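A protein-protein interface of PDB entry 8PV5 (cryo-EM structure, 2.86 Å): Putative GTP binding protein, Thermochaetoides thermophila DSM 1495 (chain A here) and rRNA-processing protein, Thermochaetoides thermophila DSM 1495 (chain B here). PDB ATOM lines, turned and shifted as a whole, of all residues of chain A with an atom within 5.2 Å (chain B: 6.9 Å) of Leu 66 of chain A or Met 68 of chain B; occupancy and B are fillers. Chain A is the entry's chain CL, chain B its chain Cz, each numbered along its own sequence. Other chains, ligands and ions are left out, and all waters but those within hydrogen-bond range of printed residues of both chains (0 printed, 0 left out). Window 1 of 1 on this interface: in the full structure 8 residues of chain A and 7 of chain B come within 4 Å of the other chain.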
ATOM      1  N   ILE A  55      27.991  20.967  20.574  1.00  0.00           N
ATOM      2  CA  ILE A  55      26.805  20.484  21.279  1.00  0.00           C
ATOM      3  C   ILE A  55      27.274  19.795  22.556  1.00  0.00           C
ATOM      4  O   ILE A  55      28.258  19.045  22.508  1.00  0.00           O
ATOM      5  CB  ILE A  55      25.992  19.514  20.401  1.00  0.00           C
ATOM      6  CG1 ILE A  55      25.605  20.179  19.081  1.00  0.00           C
ATOM      7  CG2 ILE A  55      24.712  19.097  21.095  1.00  0.00           C
ATOM      8  CD1 ILE A  55      25.039  19.215  18.063  1.00  0.00           C
ATOM      9  N   LYS A  62      21.164  14.407  21.757  1.00  0.00           N
ATOM     10  CA  LYS A  62      22.175  14.875  20.811  1.00  0.00           C
ATOM     11  C   LYS A  62      22.359  13.896  19.657  1.00  0.00           C
ATOM     12  O   LYS A  62      22.526  14.313  18.505  1.00  0.00           O
ATOM     13  CB  LYS A  62      23.505  15.103  21.529  1.00  0.00           C
ATOM     14  CG  LYS A  62      24.660  15.464  20.607  1.00  0.00           C
ATOM     15  CD  LYS A  62      25.966  15.650  21.352  1.00  0.00           C
ATOM     16  CE  LYS A  62      27.099  16.032  20.416  1.00  0.00           C
ATOM     17  NZ  LYS A  62      28.386  16.180  21.148  1.00  0.00           N
ATOM     18  N   GLU A  63      22.325  12.591  19.941  1.00  0.00           N
ATOM     19  CA  GLU A  63      22.444  11.601  18.874  1.00  0.00           C
ATOM     20  C   GLU A  63      21.271  11.702  17.904  1.00  0.00           C
ATOM     21  O   GLU A  63      21.447  11.563  16.688  1.00  0.00           O
ATOM     22  CB  GLU A  63      22.578  10.192  19.466  1.00  0.00           C
ATOM     23  CG  GLU A  63      21.382   9.652  20.259  1.00  0.00           C
ATOM     24  CD  GLU A  63      21.370  10.105  21.710  1.00  0.00           C
ATOM     25  OE1 GLU A  63      21.384   9.233  22.605  1.00  0.00           O
ATOM     26  OE2 GLU A  63      21.347  11.330  21.956  1.00  0.00           O
ATOM     27  N   ARG A  64      20.077  12.004  18.421  1.00  0.00           N
ATOM     28  CA  ARG A  64      18.927  12.255  17.558  1.00  0.00           C
ATOM     29  C   ARG A  64      19.133  13.506  16.711  1.00  0.00           C
ATOM     30  O   ARG A  64      18.774  13.526  15.527  1.00  0.00           O
ATOM     31  CB  ARG A  64      17.661  12.381  18.402  1.00  0.00           C
ATOM     32  CG  ARG A  64      17.305  11.124  19.178  1.00  0.00           C
ATOM     33  CD  ARG A  64      15.833  11.106  19.557  1.00  0.00           C
ATOM     34  NE  ARG A  64      15.467  12.239  20.401  1.00  0.00           N
ATOM     35  CZ  ARG A  64      14.609  13.185  20.045  1.00  0.00           C
ATOM     36  NH1 ARG A  64      14.012  13.170  18.865  1.00  0.00           N
ATOM     37  NH2 ARG A  64      14.347  14.174  20.895  1.00  0.00           N
ATOM     38  N   LEU A  65      19.707  14.561  17.304  1.00  0.00           N
ATOM     39  CA  LEU A  65      19.998  15.776  16.541  1.00  0.00           C
ATOM     40  C   LEU A  65      20.987  15.515  15.410  1.00  0.00           C
ATOM     41  O   LEU A  65      20.812  16.034  14.304  1.00  0.00           O
ATOM     42  CB  LEU A  65      20.512  16.889  17.458  1.00  0.00           C
ATOM     43  CG  LEU A  65      19.508  17.878  18.068  1.00  0.00           C
ATOM     44  CD1 LEU A  65      18.870  18.713  16.964  1.00  0.00           C
ATOM     45  CD2 LEU A  65      18.428  17.211  18.894  1.00  0.00           C
ATOM     46  N   LEU A  66      22.024  14.714  15.657  1.00  0.00           N
ATOM     47  CA  LEU A  66      22.931  14.348  14.567  1.00  0.00           C
ATOM     48  C   LEU A  66      22.266  13.426  13.543  1.00  0.00           C
ATOM     49  O   LEU A  66      22.621  13.465  12.357  1.00  0.00           O
ATOM     50  CB  LEU A  66      24.235  13.750  15.108  1.00  0.00           C
ATOM     51  CG  LEU A  66      25.327  14.693  15.657  1.00  0.00           C
ATOM     52  CD1 LEU A  66      25.035  15.374  16.965  1.00  0.00           C
ATOM     53  CD2 LEU A  66      26.627  13.903  15.802  1.00  0.00           C
ATOM     54  N   GLN A  67      21.280  12.620  13.963  1.00  0.00           N
ATOM     55  CA  GLN A  67      20.466  11.890  12.987  1.00  0.00           C
ATOM     56  C   GLN A  67      19.734  12.848  12.050  1.00  0.00           C
ATOM     57  O   GLN A  67      19.760  12.674  10.825  1.00  0.00           O
ATOM     58  CB  GLN A  67      19.452  10.968  13.673  1.00  0.00           C
ATOM     59  CG  GLN A  67      19.990   9.819  14.510  1.00  0.00           C
ATOM     60  CD  GLN A  67      20.714   8.777  13.685  1.00  0.00           C
ATOM     61  OE1 GLN A  67      21.729   8.232  14.114  1.00  0.00           O
ATOM     62  NE2 GLN A  67      20.231   8.540  12.470  1.00  0.00           N
ATOM     63  N   GLN A  68      19.090  13.881  12.608  1.00  0.00           N
ATOM     64  CA  GLN A  68      18.400  14.842  11.744  1.00  0.00           C
ATOM     65  C   GLN A  68      19.391  15.655  10.915  1.00  0.00           C
ATOM     66  O   GLN A  68      19.082  16.054   9.789  1.00  0.00           O
ATOM     67  CB  GLN A  68      17.472  15.788  12.521  1.00  0.00           C
ATOM     68  CG  GLN A  68      16.169  15.175  13.037  1.00  0.00           C
ATOM     69  CD  GLN A  68      16.185  14.861  14.515  1.00  0.00           C
ATOM     70  OE1 GLN A  68      16.894  15.507  15.284  1.00  0.00           O
ATOM     71  NE2 GLN A  68      15.399  13.871  14.923  1.00  0.00           N
ATOM     72  N   ILE A  69      20.593  15.899  11.450  1.00  0.00           N
ATOM     73  CA  ILE A  69      21.613  16.633  10.697  1.00  0.00           C
ATOM     74  C   ILE A  69      22.041  15.843   9.464  1.00  0.00           C
ATOM     75  O   ILE A  69      22.081  16.377   8.346  1.00  0.00           O
ATOM     76  CB  ILE A  69      22.815  16.973  11.598  1.00  0.00           C
ATOM     77  CG1 ILE A  69      22.478  18.148  12.518  1.00  0.00           C
ATOM     78  CG2 ILE A  69      24.052  17.294  10.770  1.00  0.00           C
ATOM     79  CD1 ILE A  69      23.514  18.401  13.589  1.00  0.00           C
ATOM     80  N   GLU A  70      22.336  14.551   9.645  1.00  0.00           N
ATOM     81  CA  GLU A  70      22.712  13.714   8.508  1.00  0.00           C
ATOM     82  C   GLU A  70      21.557  13.556   7.526  1.00  0.00           C
ATOM     83  O   GLU A  70      21.763  13.575   6.307  1.00  0.00           O
ATOM     84  CB  GLU A  70      23.202  12.343   8.976  1.00  0.00           C
ATOM     85  CG  GLU A  70      24.511  12.368   9.738  1.00  0.00           C
ATOM     86  CD  GLU A  70      24.941  10.987  10.187  1.00  0.00           C
ATOM     87  OE1 GLU A  70      24.154  10.033  10.014  1.00  0.00           O
ATOM     88  OE2 GLU A  70      26.072  10.850  10.695  1.00  0.00           O
ATOM     89  N   GLU A  71      20.331  13.408   8.041  1.00  0.00           N
ATOM     90  CA  GLU A  71      19.172  13.256   7.165  1.00  0.00           C
ATOM     91  C   GLU A  71      18.936  14.516   6.338  1.00  0.00           C
ATOM     92  O   GLU A  71      18.663  14.439   5.134  1.00  0.00           O
ATOM     93  CB  GLU A  71      17.936  12.904   7.995  1.00  0.00           C
ATOM     94  CG  GLU A  71      16.625  12.978   7.230  1.00  0.00           C
ATOM     95  CD  GLU A  71      15.417  12.884   8.136  1.00  0.00           C
ATOM     96  OE1 GLU A  71      15.599  12.873   9.372  1.00  0.00           O
ATOM     97  OE2 GLU A  71      14.283  12.817   7.615  1.00  0.00           O
ATOM     98  N   ARG A  73      21.216  16.788   5.570  1.00  0.00           N
ATOM     99  CA  ARG A  73      22.318  16.924   4.620  1.00  0.00           C
ATOM    100  C   ARG A  73      22.125  16.015   3.409  1.00  0.00           C
ATOM    101  O   ARG A  73      22.359  16.432   2.267  1.00  0.00           O
ATOM    102  CB  ARG A  73      23.648  16.631   5.315  1.00  0.00           C
ATOM    103  CG  ARG A  73      24.862  16.725   4.404  1.00  0.00           C
ATOM    104  CD  ARG A  73      26.096  16.132   5.062  1.00  0.00           C
ATOM    105  NE  ARG A  73      26.820  17.122   5.849  1.00  0.00           N
ATOM    106  CZ  ARG A  73      27.546  16.841   6.924  1.00  0.00           C
ATOM    107  NH1 ARG A  73      27.664  15.602   7.374  1.00  0.00           N
ATOM    108  NH2 ARG A  73      28.168  17.827   7.563  1.00  0.00           N
ATOM    109  N   MET B  61      27.930   7.258  20.678  1.00  0.00           N
ATOM    110  CA  MET B  61      27.732   8.672  20.373  1.00  0.00           C
ATOM    111  C   MET B  61      29.045   9.380  20.049  1.00  0.00           C
ATOM    112  O   MET B  61      29.142  10.109  19.050  1.00  0.00           O
ATOM    113  CB  MET B  61      27.050   9.302  21.582  1.00  0.00           C
ATOM    114  CG  MET B  61      26.657  10.743  21.526  1.00  0.00           C
ATOM    115  SD  MET B  61      25.852  10.868  23.125  1.00  0.00           S
ATOM    116  CE  MET B  61      25.437  12.599  23.212  1.00  0.00           C
ATOM    117  N   ALA B  63      31.859   7.971  19.138  1.00  0.00           N
ATOM    118  CA  ALA B  63      32.399   7.406  17.905  1.00  0.00           C
ATOM    119  C   ALA B  63      31.766   8.057  16.677  1.00  0.00           C
ATOM    120  O   ALA B  63      32.466   8.400  15.714  1.00  0.00           O
ATOM    121  CB  ALA B  63      32.191   5.893  17.884  1.00  0.00           C
ATOM    122  N   LYS B  64      30.442   8.250  16.705  1.00  0.00           N
ATOM    123  CA  LYS B  64      29.765   8.928  15.599  1.00  0.00           C
ATOM    124  C   LYS B  64      30.259  10.363  15.434  1.00  0.00           C
ATOM    125  O   LYS B  64      30.504  10.821  14.305  1.00  0.00           O
ATOM    126  CB  LYS B  64      28.254   8.926  15.830  1.00  0.00           C
ATOM    127  CG  LYS B  64      27.492   9.747  14.800  1.00  0.00           C
ATOM    128  CD  LYS B  64      25.985   9.698  14.990  1.00  0.00           C
ATOM    129  CE  LYS B  64      25.293  10.440  13.860  1.00  0.00           C
ATOM    130  NZ  LYS B  64      23.813  10.305  13.900  1.00  0.00           N
ATOM    131  N   GLU B  65      30.412  11.085  16.551  1.00  0.00           N
ATOM    132  CA  GLU B  65      30.892  12.465  16.489  1.00  0.00           C
ATOM    133  C   GLU B  65      32.302  12.536  15.917  1.00  0.00           C
ATOM    134  O   GLU B  65      32.606  13.419  15.104  1.00  0.00           O
ATOM    135  CB  GLU B  65      30.852  13.104  17.878  1.00  0.00           C
ATOM    136  CG  GLU B  65      31.361  14.538  17.921  1.00  0.00           C
ATOM    137  CD  GLU B  65      31.353  15.121  19.320  1.00  0.00           C
ATOM    138  OE1 GLU B  65      32.447  15.355  19.873  1.00  0.00           O
ATOM    139  OE2 GLU B  65      30.254  15.332  19.871  1.00  0.00           O
ATOM    140  N   ARG B  66      33.170  11.601  16.318  1.00  0.00           N
ATOM    141  CA  ARG B  66      34.534  11.573  15.799  1.00  0.00           C
ATOM    142  C   ARG B  66      34.559  11.289  14.301  1.00  0.00           C
ATOM    143  O   ARG B  66      35.320  11.922  13.560  1.00  0.00           O
ATOM    144  CB  ARG B  66      35.362  10.537  16.557  1.00  0.00           C
ATOM    145  CG  ARG B  66      36.848  10.590  16.251  1.00  0.00           C
ATOM    146  CD  ARG B  66      37.629   9.609  17.112  1.00  0.00           C
ATOM    147  NE  ARG B  66      37.527   9.932  18.531  1.00  0.00           N
ATOM    148  CZ  ARG B  66      36.928   9.168  19.435  1.00  0.00           C
ATOM    149  NH1 ARG B  66      36.362   8.018  19.104  1.00  0.00           N
ATOM    150  NH2 ARG B  66      36.896   9.567  20.704  1.00  0.00           N
ATOM    151  N   GLU B  67      33.726  10.347  13.837  1.00  0.00           N
ATOM    152  CA  GLU B  67      33.671  10.052  12.404  1.00  0.00           C
ATOM    153  C   GLU B  67      33.185  11.253  11.598  1.00  0.00           C
ATOM    154  O   GLU B  67      33.752  11.579  10.545  1.00  0.00           O
ATOM    155  CB  GLU B  67      32.781   8.834  12.138  1.00  0.00           C
ATOM    156  CG  GLU B  67      33.282   7.529  12.743  1.00  0.00           C
ATOM    157  CD  GLU B  67      34.630   7.106  12.188  1.00  0.00           C
ATOM    158  OE1 GLU B  67      34.878   7.330  10.984  1.00  0.00           O
ATOM    159  OE2 GLU B  67      35.444   6.550  12.955  1.00  0.00           O
ATOM    160  N   MET B  68      32.143  11.937  12.083  1.00  0.00           N
ATOM    161  CA  MET B  68      31.628  13.090  11.347  1.00  0.00           C
ATOM    162  C   MET B  68      32.622  14.248  11.341  1.00  0.00           C
ATOM    163  O   MET B  68      32.776  14.936  10.322  1.00  0.00           O
ATOM    164  CB  MET B  68      30.286  13.536  11.923  1.00  0.00           C
ATOM    165  CG  MET B  68      29.178  12.531  11.708  1.00  0.00           C
ATOM    166  SD  MET B  68      27.639  13.067  12.460  1.00  0.00           S
ATOM    167  CE  MET B  68      27.196  14.425  11.380  1.00  0.00           C
ATOM    168  N   LYS B  69      33.307  14.476  12.466  1.00  0.00           N
ATOM    169  CA  LYS B  69      34.307  15.537  12.515  1.00  0.00           C
ATOM    170  C   LYS B  69      35.489  15.229  11.604  1.00  0.00           C
ATOM    171  O   LYS B  69      36.023  16.131  10.950  1.00  0.00           O
ATOM    172  CB  LYS B  69      34.771  15.767  13.953  1.00  0.00           C
ATOM    173  CG  LYS B  69      33.762  16.515  14.810  1.00  0.00           C
ATOM    174  CD  LYS B  69      34.242  16.655  16.246  1.00  0.00           C
ATOM    175  CE  LYS B  69      33.325  17.569  17.045  1.00  0.00           C
ATOM    176  NZ  LYS B  69      33.739  17.673  18.473  1.00  0.00           N
ATOM    177  N   GLU B  70      35.898  13.957  11.529  1.00  0.00           N
ATOM    178  CA  GLU B  70      36.975  13.581  10.615  1.00  0.00           C
ATOM    179  C   GLU B  70      36.559  13.767   9.161  1.00  0.00           C
ATOM    180  O   GLU B  70      37.361  14.209   8.329  1.00  0.00           O
ATOM    181  CB  GLU B  70      37.406  12.138  10.870  1.00  0.00           C
ATOM    182  CG  GLU B  70      38.264  11.953  12.109  1.00  0.00           C
ATOM    183  CD  GLU B  70      38.343  10.506  12.545  1.00  0.00           C
ATOM    184  OE1 GLU B  70      37.803   9.639  11.824  1.00  0.00           O
ATOM    185  OE2 GLU B  70      38.946  10.232  13.603  1.00  0.00           O
ATOM    186  N   GLU B  71      35.303  13.441   8.835  1.00  0.00           N
ATOM    187  CA  GLU B  71      34.816  13.626   7.468  1.00  0.00           C
ATOM    188  C   GLU B  71      34.788  15.102   7.077  1.00  0.00           C
ATOM    189  O   GLU B  71      35.249  15.479   5.987  1.00  0.00           O
ATOM    190  CB  GLU B  71      33.425  13.006   7.326  1.00  0.00           C
ATOM    191  CG  GLU B  71      32.857  13.068   5.921  1.00  0.00           C
ATOM    192  CD  GLU B  71      33.551  12.117   4.969  1.00  0.00           C
ATOM    193  OE1 GLU B  71      34.062  11.075   5.433  1.00  0.00           O
ATOM    194  OE2 GLU B  71      33.585  12.411   3.756  1.00  0.00           O
ATOM    195  N   LYS B  72      34.256  15.953   7.963  1.00  0.00           N
ATOM    196  CA  LYS B  72      34.230  17.389   7.689  1.00  0.00           C
ATOM    197  C   LYS B  72      35.639  17.959   7.584  1.00  0.00           C
ATOM    198  O   LYS B  72      35.911  18.799   6.716  1.00  0.00           O
ATOM    199  CB  LYS B  72      33.432  18.122   8.767  1.00  0.00           C
ATOM    200  CG  LYS B  72      31.963  17.737   8.832  1.00  0.00           C
ATOM    201  CD  LYS B  72      31.152  18.767   9.604  1.00  0.00           C
ATOM    202  CE  LYS B  72      31.210  20.132   8.937  1.00  0.00           C
ATOM    203  NZ  LYS B  72      30.374  21.138   9.649  1.00  0.00           N
ATOM    204  N   GLU B  73      36.553  17.496   8.444  1.00  0.00           N
ATOM    205  CA  GLU B  73      37.938  17.955   8.389  1.00  0.00           C
ATOM    206  C   GLU B  73      38.604  17.555   7.078  1.00  0.00           C
ATOM    207  O   GLU B  73      39.333  18.353   6.481  1.00  0.00           O
ATOM    208  CB  GLU B  73      38.715  17.401   9.586  1.00  0.00           C
ATOM    209  CG  GLU B  73      40.226  17.625   9.540  1.00  0.00           C
ATOM    210  CD  GLU B  73      40.625  19.079   9.743  1.00  0.00           C
ATOM    211  OE1 GLU B  73      39.820  19.855  10.300  1.00  0.00           O
ATOM    212  OE2 GLU B  73      41.750  19.447   9.343  1.00  0.00           O
ATOM    213  N   ALA B  74      38.351  16.328   6.607  1.00  0.00           N
ATOM    214  CA  ALA B  74      38.922  15.876   5.341  1.00  0.00           C
ATOM    215  C   ALA B  74      38.407  16.706   4.171  1.00  0.00           C
ATOM    216  O   ALA B  74      39.175  17.080   3.274  1.00  0.00           O
ATOM    217  CB  ALA B  74      38.616  14.393   5.130  1.00  0.00           C
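The side-chain amide oxygen (OE1) of Gln 67 of chain A lies within hydrogen-bond range of the side-chain amino group (NZ) of Lys 64 of chain B, 2.9 Å away.
The side-chain sulfur (SD) of Met 68 of chain B sits close to the side-chain carboxylate (OE2) of Glu 70 of chain A (3.2 Å).
OE2 of Glu 65 of chain B is in salt-bridge range of NZ of Lys 62 of chain A, at 2.4 Å.
The side-chain carboxylate (OE1) of Glu 70 of chain A lies within salt-bridge range of the side-chain amino group (NZ) of Lys 64 of chain B, at 3.9 Å.
NZ of Lys 62 of chain A lies within hydrogen-bond range of O of Ile 55 of chain A (3.2 Å).
OE1 of Glu 65 of chain B is in salt-bridge range of NZ of Lys 69 of chain B (3.0 Å).
Lys 62 of chain A touches Met 61 of chain B (CB to CE, 3.6 Å).
Glu 63 of chain A touches Lys 64 of chain B.
Leu 66 of chain A touches Lys 64 of chain B (C to NZ, 3.5 Å).
Met 68 of chain B touches Leu 66 of chain A.
Arg 73 of chain A touches Lys 72 of chain B (NH2 to CD, 3.7 Å).
Printed residues of chain B within 4 Å of Leu 66 of chain A: Lys 64 (3.5 Å) and Met 68 (3.6 Å).
Met 68 of chain B touches just these residues of chain A: Leu 66 and Glu 70.
Of the printed residues of chain B, Arg 73 of chain A touches Lys 72 (3.7 Å).
Printed residues of chain B within 4 Å of Gln 67 of chain A: Lys 64 (2.9 Å).
Printed residues of chain A within 4 Å of Met 61 of chain B: Lys 62.
Glu 73 of chain B touches none of the printed residues of chain A.
Ile 69 of chain A touches none of the printed residues of chain B.
The nearest residue of chain B that does not touch Leu 66 of chain A is Glu 65 of chain B (4.6 Å).
The nearest printed residue of chain B that does not touch Arg 73 of chain A is Met 68 of chain B (4.2 Å).
Printed residues of chain A that touch a printed residue of chain B: Lys 62, Glu 63, Leu 66, Gln 67, Glu 70 and Arg 73.
Hydrophobic or aromatic side chains of chain A that line the printed part of chain B: Leu 66.
Along chain A the printed residues that touch a printed residue of chain B span positions 62 to 73.
Of the 13 printed residues of chain B, 5 touch a printed residue of chain A.
Printed residues of chain B that touch a printed residue of chain A: Met 61, Lys 64, Glu 65, Met 68 and Lys 72.
Among the printed residues, 9 pairs touch across the chains.
Among the printed residues, Asp or Glu carboxylates within 4 Å of a Lys or Arg side-chain nitrogen of the other chain: Lys 62 of chain A with Glu 65 of chain B (2.4 Å) and Glu 70 of chain A with Lys 64 of chain B (3.9 Å).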
